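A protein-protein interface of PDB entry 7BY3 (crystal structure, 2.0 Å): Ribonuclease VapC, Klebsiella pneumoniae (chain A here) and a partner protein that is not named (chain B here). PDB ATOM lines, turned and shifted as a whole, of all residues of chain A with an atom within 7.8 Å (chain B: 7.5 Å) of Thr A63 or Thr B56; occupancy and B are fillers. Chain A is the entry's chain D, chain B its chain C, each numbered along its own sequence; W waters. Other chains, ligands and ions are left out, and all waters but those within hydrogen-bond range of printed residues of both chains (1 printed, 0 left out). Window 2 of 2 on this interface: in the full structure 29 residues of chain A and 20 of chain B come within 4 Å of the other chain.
O of Ala B60 sits close to O of Leu A16, 3.3 Å away.
The side-chain hydroxyl (OG1) of Thr B56 lies within hydrogen-bond range of the backbone carbonyl oxygen (O) of Arg B52, 3.1 Å away.
The side-chain hydroxyl (OG1) of Thr A63 sits at hydrogen-bond distance from the backbone carbonyl oxygen (O) of Ala A60 (2.6 Å).
Leu A16 touches Ile B57.
CA of Leu B61 touches O of Leu A16, at 3.6 Å.
Ala B60 touches Phe A17 (O to CA, 3.3 Å).
Gln B50 touches Pro A32 (OE1 to CD, 3.3 Å).
CG2 of Thr B56 touches CG2 of Thr A63 (3.6 Å).
Of the printed residues of chain B, Phe A17 touches Ala B60 (3.3 Å).
Printed residues of chain B within 4 Å of Pro A32: Gln B50 (3.3 Å).
Leu A61 touches none of the printed residues of chain B.
Of chain B, only Thr B56 (3.6 Å) comes within 4 Å of Thr A63.
Thr B56 touches just one residue of chain A: Thr A63.
Ser B59 touches none of the printed residues of chain A.
The nearest printed residue of chain A that does not touch Gln B50 is Gln A33 (7.1 Å).
Of the 12 printed residues of chain B, 5 touch a printed residue of chain A.
Printed residues of chain B that touch a printed residue of chain A: Gln B50, Thr B56, Ile B57, Ala B60 and Leu B61.
Of the 19 printed residues of chain A, 4 touch a printed residue of chain B.
Printed residues of chain A that touch a printed residue of chain B: Leu A16, Phe A17, Pro A32 and Thr A63.
Among the printed residues, 6 pairs touch across the chains.
Among the printed residues, no Asp or Glu carboxylate lies within 4 Å of a Lys or Arg side-chain nitrogen of the other chain.
Water W1 lies within hydrogen-bond range of the backbone carbonyl oxygen of Pro A32 and the side-chain amide nitrogen of Gln B50.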
ATOM      1  N   LEU A  13       1.216 -21.829  34.894  1.00  0.00           N
ATOM      2  CA  LEU A  13       0.847 -22.945  34.032  1.00  0.00           C
ATOM      3  C   LEU A  13       0.307 -24.119  34.848  1.00  0.00           C
ATOM      4  O   LEU A  13      -0.636 -24.788  34.428  1.00  0.00           O
ATOM      5  CB  LEU A  13       2.040 -23.388  33.180  1.00  0.00           C
ATOM      6  CG  LEU A  13       2.042 -22.897  31.729  1.00  0.00           C
ATOM      7  CD1 LEU A  13       3.336 -23.266  31.036  1.00  0.00           C
ATOM      8  CD2 LEU A  13       0.861 -23.475  30.970  1.00  0.00           C
ATOM      9  N   LEU A  16      -3.173 -23.397  35.787  1.00  0.00           N
ATOM     10  CA  LEU A  16      -4.052 -23.543  34.633  1.00  0.00           C
ATOM     11  C   LEU A  16      -4.518 -24.982  34.462  1.00  0.00           C
ATOM     12  O   LEU A  16      -5.716 -25.250  34.381  1.00  0.00           O
ATOM     13  CB  LEU A  16      -3.350 -23.075  33.359  1.00  0.00           C
ATOM     14  CG  LEU A  16      -4.154 -23.277  32.073  1.00  0.00           C
ATOM     15  CD1 LEU A  16      -5.432 -22.449  32.100  1.00  0.00           C
ATOM     16  CD2 LEU A  16      -3.316 -22.950  30.851  1.00  0.00           C
ATOM     17  N   PHE A  17      -3.565 -25.908  34.407  1.00  0.00           N
ATOM     18  CA  PHE A  17      -3.885 -27.321  34.249  1.00  0.00           C
ATOM     19  C   PHE A  17      -4.601 -27.861  35.482  1.00  0.00           C
ATOM     20  O   PHE A  17      -5.318 -28.858  35.406  1.00  0.00           O
ATOM     21  CB  PHE A  17      -2.618 -28.137  33.977  1.00  0.00           C
ATOM     22  CG  PHE A  17      -1.937 -27.789  32.684  1.00  0.00           C
ATOM     23  CD1 PHE A  17      -2.568 -28.013  31.470  1.00  0.00           C
ATOM     24  CD2 PHE A  17      -0.662 -27.251  32.679  1.00  0.00           C
ATOM     25  CE1 PHE A  17      -1.941 -27.697  30.280  1.00  0.00           C
ATOM     26  CE2 PHE A  17      -0.031 -26.932  31.492  1.00  0.00           C
ATOM     27  CZ  PHE A  17      -0.671 -27.156  30.291  1.00  0.00           C
ATOM     28  N   PRO A  32      -0.823 -13.736  22.107  1.00  0.00           N
ATOM     29  CA  PRO A  32      -0.111 -14.871  21.517  1.00  0.00           C
ATOM     30  C   PRO A  32       0.831 -14.369  20.436  1.00  0.00           C
ATOM     31  O   PRO A  32       0.510 -13.351  19.825  1.00  0.00           O
ATOM     32  CB  PRO A  32      -1.236 -15.712  20.916  1.00  0.00           C
ATOM     33  CG  PRO A  32      -2.273 -14.707  20.549  1.00  0.00           C
ATOM     34  CD  PRO A  32      -2.205 -13.633  21.607  1.00  0.00           C
ATOM     35  N   GLN A  33       1.959 -15.029  20.190  1.00  0.00           N
ATOM     36  CA  GLN A  33       2.411 -16.227  20.889  1.00  0.00           C
ATOM     37  C   GLN A  33       3.153 -15.886  22.175  1.00  0.00           C
ATOM     38  O   GLN A  33       4.015 -15.009  22.177  1.00  0.00           O
ATOM     39  CB  GLN A  33       3.312 -17.032  19.940  1.00  0.00           C
ATOM     40  CG  GLN A  33       3.889 -18.347  20.456  1.00  0.00           C
ATOM     41  CD  GLN A  33       4.902 -18.951  19.479  1.00  0.00           C
ATOM     42  OE1 GLN A  33       6.110 -18.809  19.650  1.00  0.00           O
ATOM     43  NE2 GLN A  33       4.406 -19.636  18.459  1.00  0.00           N
ATOM     44  N   ASN A  34       2.825 -16.571  23.265  1.00  0.00           N
ATOM     45  CA  ASN A  34       3.558 -16.359  24.506  1.00  0.00           C
ATOM     46  C   ASN A  34       4.697 -17.361  24.641  1.00  0.00           C
ATOM     47  O   ASN A  34       4.859 -18.244  23.800  1.00  0.00           O
ATOM     48  CB  ASN A  34       2.624 -16.444  25.714  1.00  0.00           C
ATOM     49  CG  ASN A  34       1.747 -15.211  25.863  1.00  0.00           C
ATOM     50  OD1 ASN A  34       2.214 -14.078  25.722  1.00  0.00           O
ATOM     51  ND2 ASN A  34       0.466 -15.428  26.141  1.00  0.00           N
ATOM     52  N   ALA A  35       5.477 -17.237  25.708  1.00  0.00           N
ATOM     53  CA  ALA A  35       6.680 -18.047  25.846  1.00  0.00           C
ATOM     54  C   ALA A  35       6.859 -18.649  27.235  1.00  0.00           C
ATOM     55  O   ALA A  35       6.366 -18.123  28.232  1.00  0.00           O
ATOM     56  CB  ALA A  35       7.904 -17.218  25.482  1.00  0.00           C
ATOM     57  N   ILE A  36       7.563 -19.776  27.275  1.00  0.00           N
ATOM     58  CA  ILE A  36       8.006 -20.383  28.521  1.00  0.00           C
ATOM     59  C   ILE A  36       9.472 -20.774  28.390  1.00  0.00           C
ATOM     60  O   ILE A  36       9.982 -20.932  27.282  1.00  0.00           O
ATOM     61  CB  ILE A  36       7.179 -21.634  28.894  1.00  0.00           C
ATOM     62  CG1 ILE A  36       7.307 -22.707  27.810  1.00  0.00           C
ATOM     63  CG2 ILE A  36       5.722 -21.273  29.123  1.00  0.00           C
ATOM     64  CD1 ILE A  36       6.687 -24.031  28.192  1.00  0.00           C
ATOM     65  N   ARG A  56      -1.637 -34.680  26.171  1.00  0.00           N
ATOM     66  CA  ARG A  56      -2.417 -33.467  25.934  1.00  0.00           C
ATOM     67  C   ARG A  56      -1.771 -32.239  26.568  1.00  0.00           C
ATOM     68  O   ARG A  56      -1.974 -31.118  26.105  1.00  0.00           O
ATOM     69  CB  ARG A  56      -3.850 -33.634  26.449  1.00  0.00           C
ATOM     70  CG  ARG A  56      -4.709 -34.545  25.587  1.00  0.00           C
ATOM     71  CD  ARG A  56      -6.193 -34.407  25.900  1.00  0.00           C
ATOM     72  NE  ARG A  56      -6.993 -35.321  25.087  1.00  0.00           N
ATOM     73  CZ  ARG A  56      -8.275 -35.598  25.303  1.00  0.00           C
ATOM     74  NH1 ARG A  56      -8.921 -35.030  26.312  1.00  0.00           N
ATOM     75  NH2 ARG A  56      -8.913 -36.444  24.505  1.00  0.00           N
ATOM     76  N   THR A  57      -0.995 -32.453  27.626  1.00  0.00           N
ATOM     77  CA  THR A  57      -0.231 -31.369  28.230  1.00  0.00           C
ATOM     78  C   THR A  57       0.883 -30.940  27.287  1.00  0.00           C
ATOM     79  O   THR A  57       1.172 -29.751  27.146  1.00  0.00           O
ATOM     80  CB  THR A  57       0.372 -31.780  29.582  1.00  0.00           C
ATOM     81  OG1 THR A  57      -0.676 -32.189  30.468  1.00  0.00           O
ATOM     82  CG2 THR A  57       1.134 -30.618  30.204  1.00  0.00           C
ATOM     83  N   ARG A  58       1.495 -31.923  26.634  1.00  0.00           N
ATOM     84  CA  ARG A  58       2.552 -31.666  25.665  1.00  0.00           C
ATOM     85  C   ARG A  58       2.018 -30.849  24.490  1.00  0.00           C
ATOM     86  O   ARG A  58       2.748 -30.064  23.886  1.00  0.00           O
ATOM     87  CB  ARG A  58       3.156 -32.984  25.169  1.00  0.00           C
ATOM     88  CG  ARG A  58       4.524 -32.843  24.511  1.00  0.00           C
ATOM     89  CD  ARG A  58       5.036 -34.177  23.977  1.00  0.00           C
ATOM     90  NE  ARG A  58       6.147 -34.706  24.766  1.00  0.00           N
ATOM     91  CZ  ARG A  58       6.041 -35.710  25.632  1.00  0.00           C
ATOM     92  NH1 ARG A  58       4.873 -36.305  25.821  1.00  0.00           N
ATOM     93  NH2 ARG A  58       7.104 -36.124  26.304  1.00  0.00           N
ATOM     94  N   MET A  59       0.739 -31.032  24.176  1.00  0.00           N
ATOM     95  CA  MET A  59       0.118 -30.321  23.063  1.00  0.00           C
ATOM     96  C   MET A  59      -0.258 -28.890  23.429  1.00  0.00           C
ATOM     97  O   MET A  59      -0.266 -28.008  22.573  1.00  0.00           O
ATOM     98  CB  MET A  59      -1.112 -31.079  22.564  1.00  0.00           C
ATOM     99  CG  MET A  59      -0.768 -32.188  21.579  1.00  0.00           C
ATOM    100  SD  MET A  59      -2.194 -32.958  20.794  1.00  0.00           S
ATOM    101  CE  MET A  59      -2.560 -34.270  21.955  1.00  0.00           C
ATOM    102  N   ALA A  60      -0.572 -28.660  24.698  1.00  0.00           N
ATOM    103  CA  ALA A  60      -0.878 -27.314  25.165  1.00  0.00           C
ATOM    104  C   ALA A  60       0.394 -26.479  25.262  1.00  0.00           C
ATOM    105  O   ALA A  60       0.395 -25.291  24.945  1.00  0.00           O
ATOM    106  CB  ALA A  60      -1.585 -27.363  26.506  1.00  0.00           C
ATOM    107  N   LEU A  61       1.477 -27.114  25.700  1.00  0.00           N
ATOM    108  CA  LEU A  61       2.763 -26.441  25.845  1.00  0.00           C
ATOM    109  C   LEU A  61       3.360 -26.054  24.496  1.00  0.00           C
ATOM    110  O   LEU A  61       4.146 -25.112  24.403  1.00  0.00           O
ATOM    111  CB  LEU A  61       3.744 -27.336  26.607  1.00  0.00           C
ATOM    112  CG  LEU A  61       3.513 -27.495  28.110  1.00  0.00           C
ATOM    113  CD1 LEU A  61       4.430 -28.557  28.675  1.00  0.00           C
ATOM    114  CD2 LEU A  61       3.733 -26.177  28.829  1.00  0.00           C
ATOM    115  N   SER A  62       2.978 -26.784  23.452  1.00  0.00           N
ATOM    116  CA  SER A  62       3.549 -26.591  22.123  1.00  0.00           C
ATOM    117  C   SER A  62       3.095 -25.286  21.476  1.00  0.00           C
ATOM    118  O   SER A  62       3.724 -24.804  20.534  1.00  0.00           O
ATOM    119  CB  SER A  62       3.192 -27.770  21.218  1.00  0.00           C
ATOM    120  OG  SER A  62       1.825 -27.732  20.846  1.00  0.00           O
ATOM    121  N   THR A  63       2.003 -24.722  21.980  1.00  0.00           N
ATOM    122  CA  THR A  63       1.495 -23.451  21.472  1.00  0.00           C
ATOM    123  C   THR A  63       2.383 -22.296  21.927  1.00  0.00           C
ATOM    124  O   THR A  63       2.410 -21.234  21.308  1.00  0.00           O
ATOM    125  CB  THR A  63       0.050 -23.197  21.932  1.00  0.00           C
ATOM    126  OG1 THR A  63      -0.028 -23.323  23.358  1.00  0.00           O
ATOM    127  CG2 THR A  63      -0.890 -24.206  21.293  1.00  0.00           C
ATOM    128  N   PHE A  64       3.094 -22.516  23.026  1.00  0.00           N
ATOM    129  CA  PHE A  64       4.060 -21.558  23.552  1.00  0.00           C
ATOM    130  C   PHE A  64       5.347 -21.535  22.738  1.00  0.00           C
ATOM    131  O   PHE A  64       5.628 -22.457  21.974  1.00  0.00           O
ATOM    132  CB  PHE A  64       4.390 -21.874  25.014  1.00  0.00           C
ATOM    133  CG  PHE A  64       3.237 -21.679  25.954  1.00  0.00           C
ATOM    134  CD1 PHE A  64       2.265 -22.654  26.092  1.00  0.00           C
ATOM    135  CD2 PHE A  64       3.128 -20.521  26.702  1.00  0.00           C
ATOM    136  CE1 PHE A  64       1.203 -22.476  26.956  1.00  0.00           C
ATOM    137  CE2 PHE A  64       2.071 -20.337  27.568  1.00  0.00           C
ATOM    138  CZ  PHE A  64       1.106 -21.316  27.696  1.00  0.00           C
ATOM    139  N   ASN A  65       6.128 -20.475  22.909  1.00  0.00           N
ATOM    140  CA  ASN A  65       7.487 -20.466  22.396  1.00  0.00           C
ATOM    141  C   ASN A  65       8.385 -21.027  23.479  1.00  0.00           C
ATOM    142  O   ASN A  65       8.595 -20.396  24.513  1.00  0.00           O
ATOM    143  CB  ASN A  65       7.938 -19.057  22.014  1.00  0.00           C
ATOM    144  CG  ASN A  65       9.362 -19.020  21.499  1.00  0.00           C
ATOM    145  OD1 ASN A  65       9.876 -20.015  20.991  1.00  0.00           O
ATOM    146  ND2 ASN A  65      10.007 -17.867  21.628  1.00  0.00           N
ATOM    147  N   ILE A  66       8.922 -22.214  23.239  1.00  0.00           N
ATOM    148  CA  ILE A  66       9.725 -22.871  24.252  1.00  0.00           C
ATOM    149  C   ILE A  66      11.173 -22.489  24.020  1.00  0.00           C
ATOM    150  O   ILE A  66      11.795 -22.905  23.043  1.00  0.00           O
ATOM    151  CB  ILE A  66       9.540 -24.394  24.219  1.00  0.00           C
ATOM    152  CG1 ILE A  66       8.049 -24.732  24.265  1.00  0.00           C
ATOM    153  CG2 ILE A  66      10.268 -25.043  25.382  1.00  0.00           C
ATOM    154  CD1 ILE A  66       7.739 -26.177  23.981  1.00  0.00           C
ATOM    155  N   GLN B  50      -6.254 -14.643  18.197  1.00  0.00           N
ATOM    156  CA  GLN B  50      -6.677 -14.572  19.593  1.00  0.00           C
ATOM    157  C   GLN B  50      -7.639 -15.709  19.929  1.00  0.00           C
ATOM    158  O   GLN B  50      -7.614 -16.248  21.034  1.00  0.00           O
ATOM    159  CB  GLN B  50      -7.337 -13.223  19.888  1.00  0.00           C
ATOM    160  CG  GLN B  50      -6.606 -12.027  19.300  1.00  0.00           C
ATOM    161  CD  GLN B  50      -5.187 -11.892  19.812  1.00  0.00           C
ATOM    162  OE1 GLN B  50      -4.954 -11.816  21.018  1.00  0.00           O
ATOM    163  NE2 GLN B  50      -4.227 -11.862  18.895  1.00  0.00           N
ATOM    164  N   ASP B  51      -8.483 -16.062  18.964  1.00  0.00           N
ATOM    165  CA  ASP B  51      -9.441 -17.153  19.124  1.00  0.00           C
ATOM    166  C   ASP B  51      -8.740 -18.485  19.367  1.00  0.00           C
ATOM    167  O   ASP B  51      -9.143 -19.256  20.238  1.00  0.00           O
ATOM    168  CB  ASP B  51     -10.344 -17.261  17.892  1.00  0.00           C
ATOM    169  CG  ASP B  51     -11.531 -16.316  17.947  1.00  0.00           C
ATOM    170  OD1 ASP B  51     -11.392 -15.210  18.511  1.00  0.00           O
ATOM    171  OD2 ASP B  51     -12.605 -16.681  17.421  1.00  0.00           O
ATOM    172  N   ARG B  52      -7.695 -18.748  18.587  1.00  0.00           N
ATOM    173  CA  ARG B  52      -6.912 -19.972  18.725  1.00  0.00           C
ATOM    174  C   ARG B  52      -6.332 -20.112  20.129  1.00  0.00           C
ATOM    175  O   ARG B  52      -6.363 -21.193  20.716  1.00  0.00           O
ATOM    176  CB  ARG B  52      -5.783 -20.007  17.691  1.00  0.00           C
ATOM    177  CG  ARG B  52      -6.093 -20.831  16.452  1.00  0.00           C
ATOM    178  CD  ARG B  52      -4.849 -21.042  15.602  1.00  0.00           C
ATOM    179  NE  ARG B  52      -4.330 -19.789  15.061  1.00  0.00           N
ATOM    180  CZ  ARG B  52      -4.713 -19.261  13.903  1.00  0.00           C
ATOM    181  NH1 ARG B  52      -5.622 -19.877  13.160  1.00  0.00           N
ATOM    182  NH2 ARG B  52      -4.187 -18.116  13.487  1.00  0.00           N
ATOM    183  N   ALA B  53      -5.806 -19.011  20.659  1.00  0.00           N
ATOM    184  CA  ALA B  53      -5.239 -19.001  22.003  1.00  0.00           C
ATOM    185  C   ALA B  53      -6.305 -19.321  23.042  1.00  0.00           C
ATOM    186  O   ALA B  53      -6.089 -20.140  23.936  1.00  0.00           O
ATOM    187  CB  ALA B  53      -4.597 -17.655  22.299  1.00  0.00           C
ATOM    188  N   LYS B  54      -7.456 -18.668  22.912  1.00  0.00           N
ATOM    189  CA  LYS B  54      -8.583 -18.884  23.811  1.00  0.00           C
ATOM    190  C   LYS B  54      -9.006 -20.349  23.817  1.00  0.00           C
ATOM    191  O   LYS B  54      -9.370 -20.897  24.858  1.00  0.00           O
ATOM    192  CB  LYS B  54      -9.760 -17.988  23.408  1.00  0.00           C
ATOM    193  CG  LYS B  54     -11.106 -18.692  23.352  1.00  0.00           C
ATOM    194  CD  LYS B  54     -12.236 -17.720  23.067  1.00  0.00           C
ATOM    195  CE  LYS B  54     -13.529 -18.461  22.771  1.00  0.00           C
ATOM    196  NZ  LYS B  54     -14.730 -17.614  23.011  1.00  0.00           N
ATOM    197  N   ASP B  55      -8.942 -20.979  22.648  1.00  0.00           N
ATOM    198  CA  ASP B  55      -9.309 -22.382  22.503  1.00  0.00           C
ATOM    199  C   ASP B  55      -8.350 -23.282  23.277  1.00  0.00           C
ATOM    200  O   ASP B  55      -8.775 -24.110  24.083  1.00  0.00           O
ATOM    201  CB  ASP B  55      -9.328 -22.779  21.025  1.00  0.00           C
ATOM    202  CG  ASP B  55      -9.972 -24.132  20.790  1.00  0.00           C
ATOM    203  OD1 ASP B  55      -9.307 -25.162  21.033  1.00  0.00           O
ATOM    204  OD2 ASP B  55     -11.142 -24.165  20.359  1.00  0.00           O
ATOM    205  N   THR B  56      -7.057 -23.107  23.021  1.00  0.00           N
ATOM    206  CA  THR B  56      -6.017 -23.903  23.663  1.00  0.00           C
ATOM    207  C   THR B  56      -6.072 -23.798  25.182  1.00  0.00           C
ATOM    208  O   THR B  56      -6.015 -24.805  25.889  1.00  0.00           O
ATOM    209  CB  THR B  56      -4.615 -23.473  23.188  1.00  0.00           C
ATOM    210  OG1 THR B  56      -4.558 -23.511  21.757  1.00  0.00           O
ATOM    211  CG2 THR B  56      -3.550 -24.392  23.765  1.00  0.00           C
ATOM    212  N   ILE B  57      -6.191 -22.570  25.675  1.00  0.00           N
ATOM    213  CA  ILE B  57      -6.211 -22.306  27.108  1.00  0.00           C
ATOM    214  C   ILE B  57      -7.442 -22.920  27.777  1.00  0.00           C
ATOM    215  O   ILE B  57      -7.375 -23.389  28.913  1.00  0.00           O
ATOM    216  CB  ILE B  57      -6.162 -20.789  27.378  1.00  0.00           C
ATOM    217  CG1 ILE B  57      -4.844 -20.212  26.859  1.00  0.00           C
ATOM    218  CG2 ILE B  57      -6.317 -20.487  28.860  1.00  0.00           C
ATOM    219  CD1 ILE B  57      -4.702 -18.726  27.068  1.00  0.00           C
ATOM    220  N   SER B  58      -8.560 -22.938  27.058  1.00  0.00           N
ATOM    221  CA  SER B  58      -9.811 -23.447  27.610  1.00  0.00           C
ATOM    222  C   SER B  58      -9.795 -24.965  27.796  1.00  0.00           C
ATOM    223  O   SER B  58     -10.377 -25.485  28.748  1.00  0.00           O
ATOM    224  CB  SER B  58     -10.987 -23.041  26.720  1.00  0.00           C
ATOM    225  OG  SER B  58     -11.210 -21.644  26.783  1.00  0.00           O
ATOM    226  N   SER B  59      -9.131 -25.673  26.887  1.00  0.00           N
ATOM    227  CA  SER B  59      -9.036 -27.127  26.982  1.00  0.00           C
ATOM    228  C   SER B  59      -7.977 -27.542  27.997  1.00  0.00           C
ATOM    229  O   SER B  59      -7.984 -28.669  28.491  1.00  0.00           O
ATOM    230  CB  SER B  59      -8.728 -27.739  25.616  1.00  0.00           C
ATOM    231  OG  SER B  59      -9.863 -27.687  24.769  1.00  0.00           O
ATOM    232  N   ALA B  60      -7.069 -26.624  28.309  1.00  0.00           N
ATOM    233  CA  ALA B  60      -6.044 -26.882  29.309  1.00  0.00           C
ATOM    234  C   ALA B  60      -6.619 -26.728  30.712  1.00  0.00           C
ATOM    235  O   ALA B  60      -6.021 -27.171  31.690  1.00  0.00           O
ATOM    236  CB  ALA B  60      -4.867 -25.946  29.114  1.00  0.00           C
ATOM    237  N   LEU B  61      -7.791 -26.105  30.796  1.00  0.00           N
ATOM    238  CA  LEU B  61      -8.397 -25.769  32.079  1.00  0.00           C
ATOM    239  C   LEU B  61      -9.600 -26.620  32.481  1.00  0.00           C
ATOM    240  O   LEU B  61     -10.600 -26.676  31.768  1.00  0.00           O
ATOM    241  CB  LEU B  61      -8.835 -24.302  32.073  1.00  0.00           C
ATOM    242  CG  LEU B  61      -9.615 -23.847  33.313  1.00  0.00           C
ATOM    243  CD1 LEU B  61      -8.738 -23.052  34.261  1.00  0.00           C
ATOM    244  CD2 LEU B  61     -10.854 -23.055  32.920  1.00  0.00           C
HETATM  245  O   HOH W   1      -1.333 -11.188  19.120  1.00  0.00           O
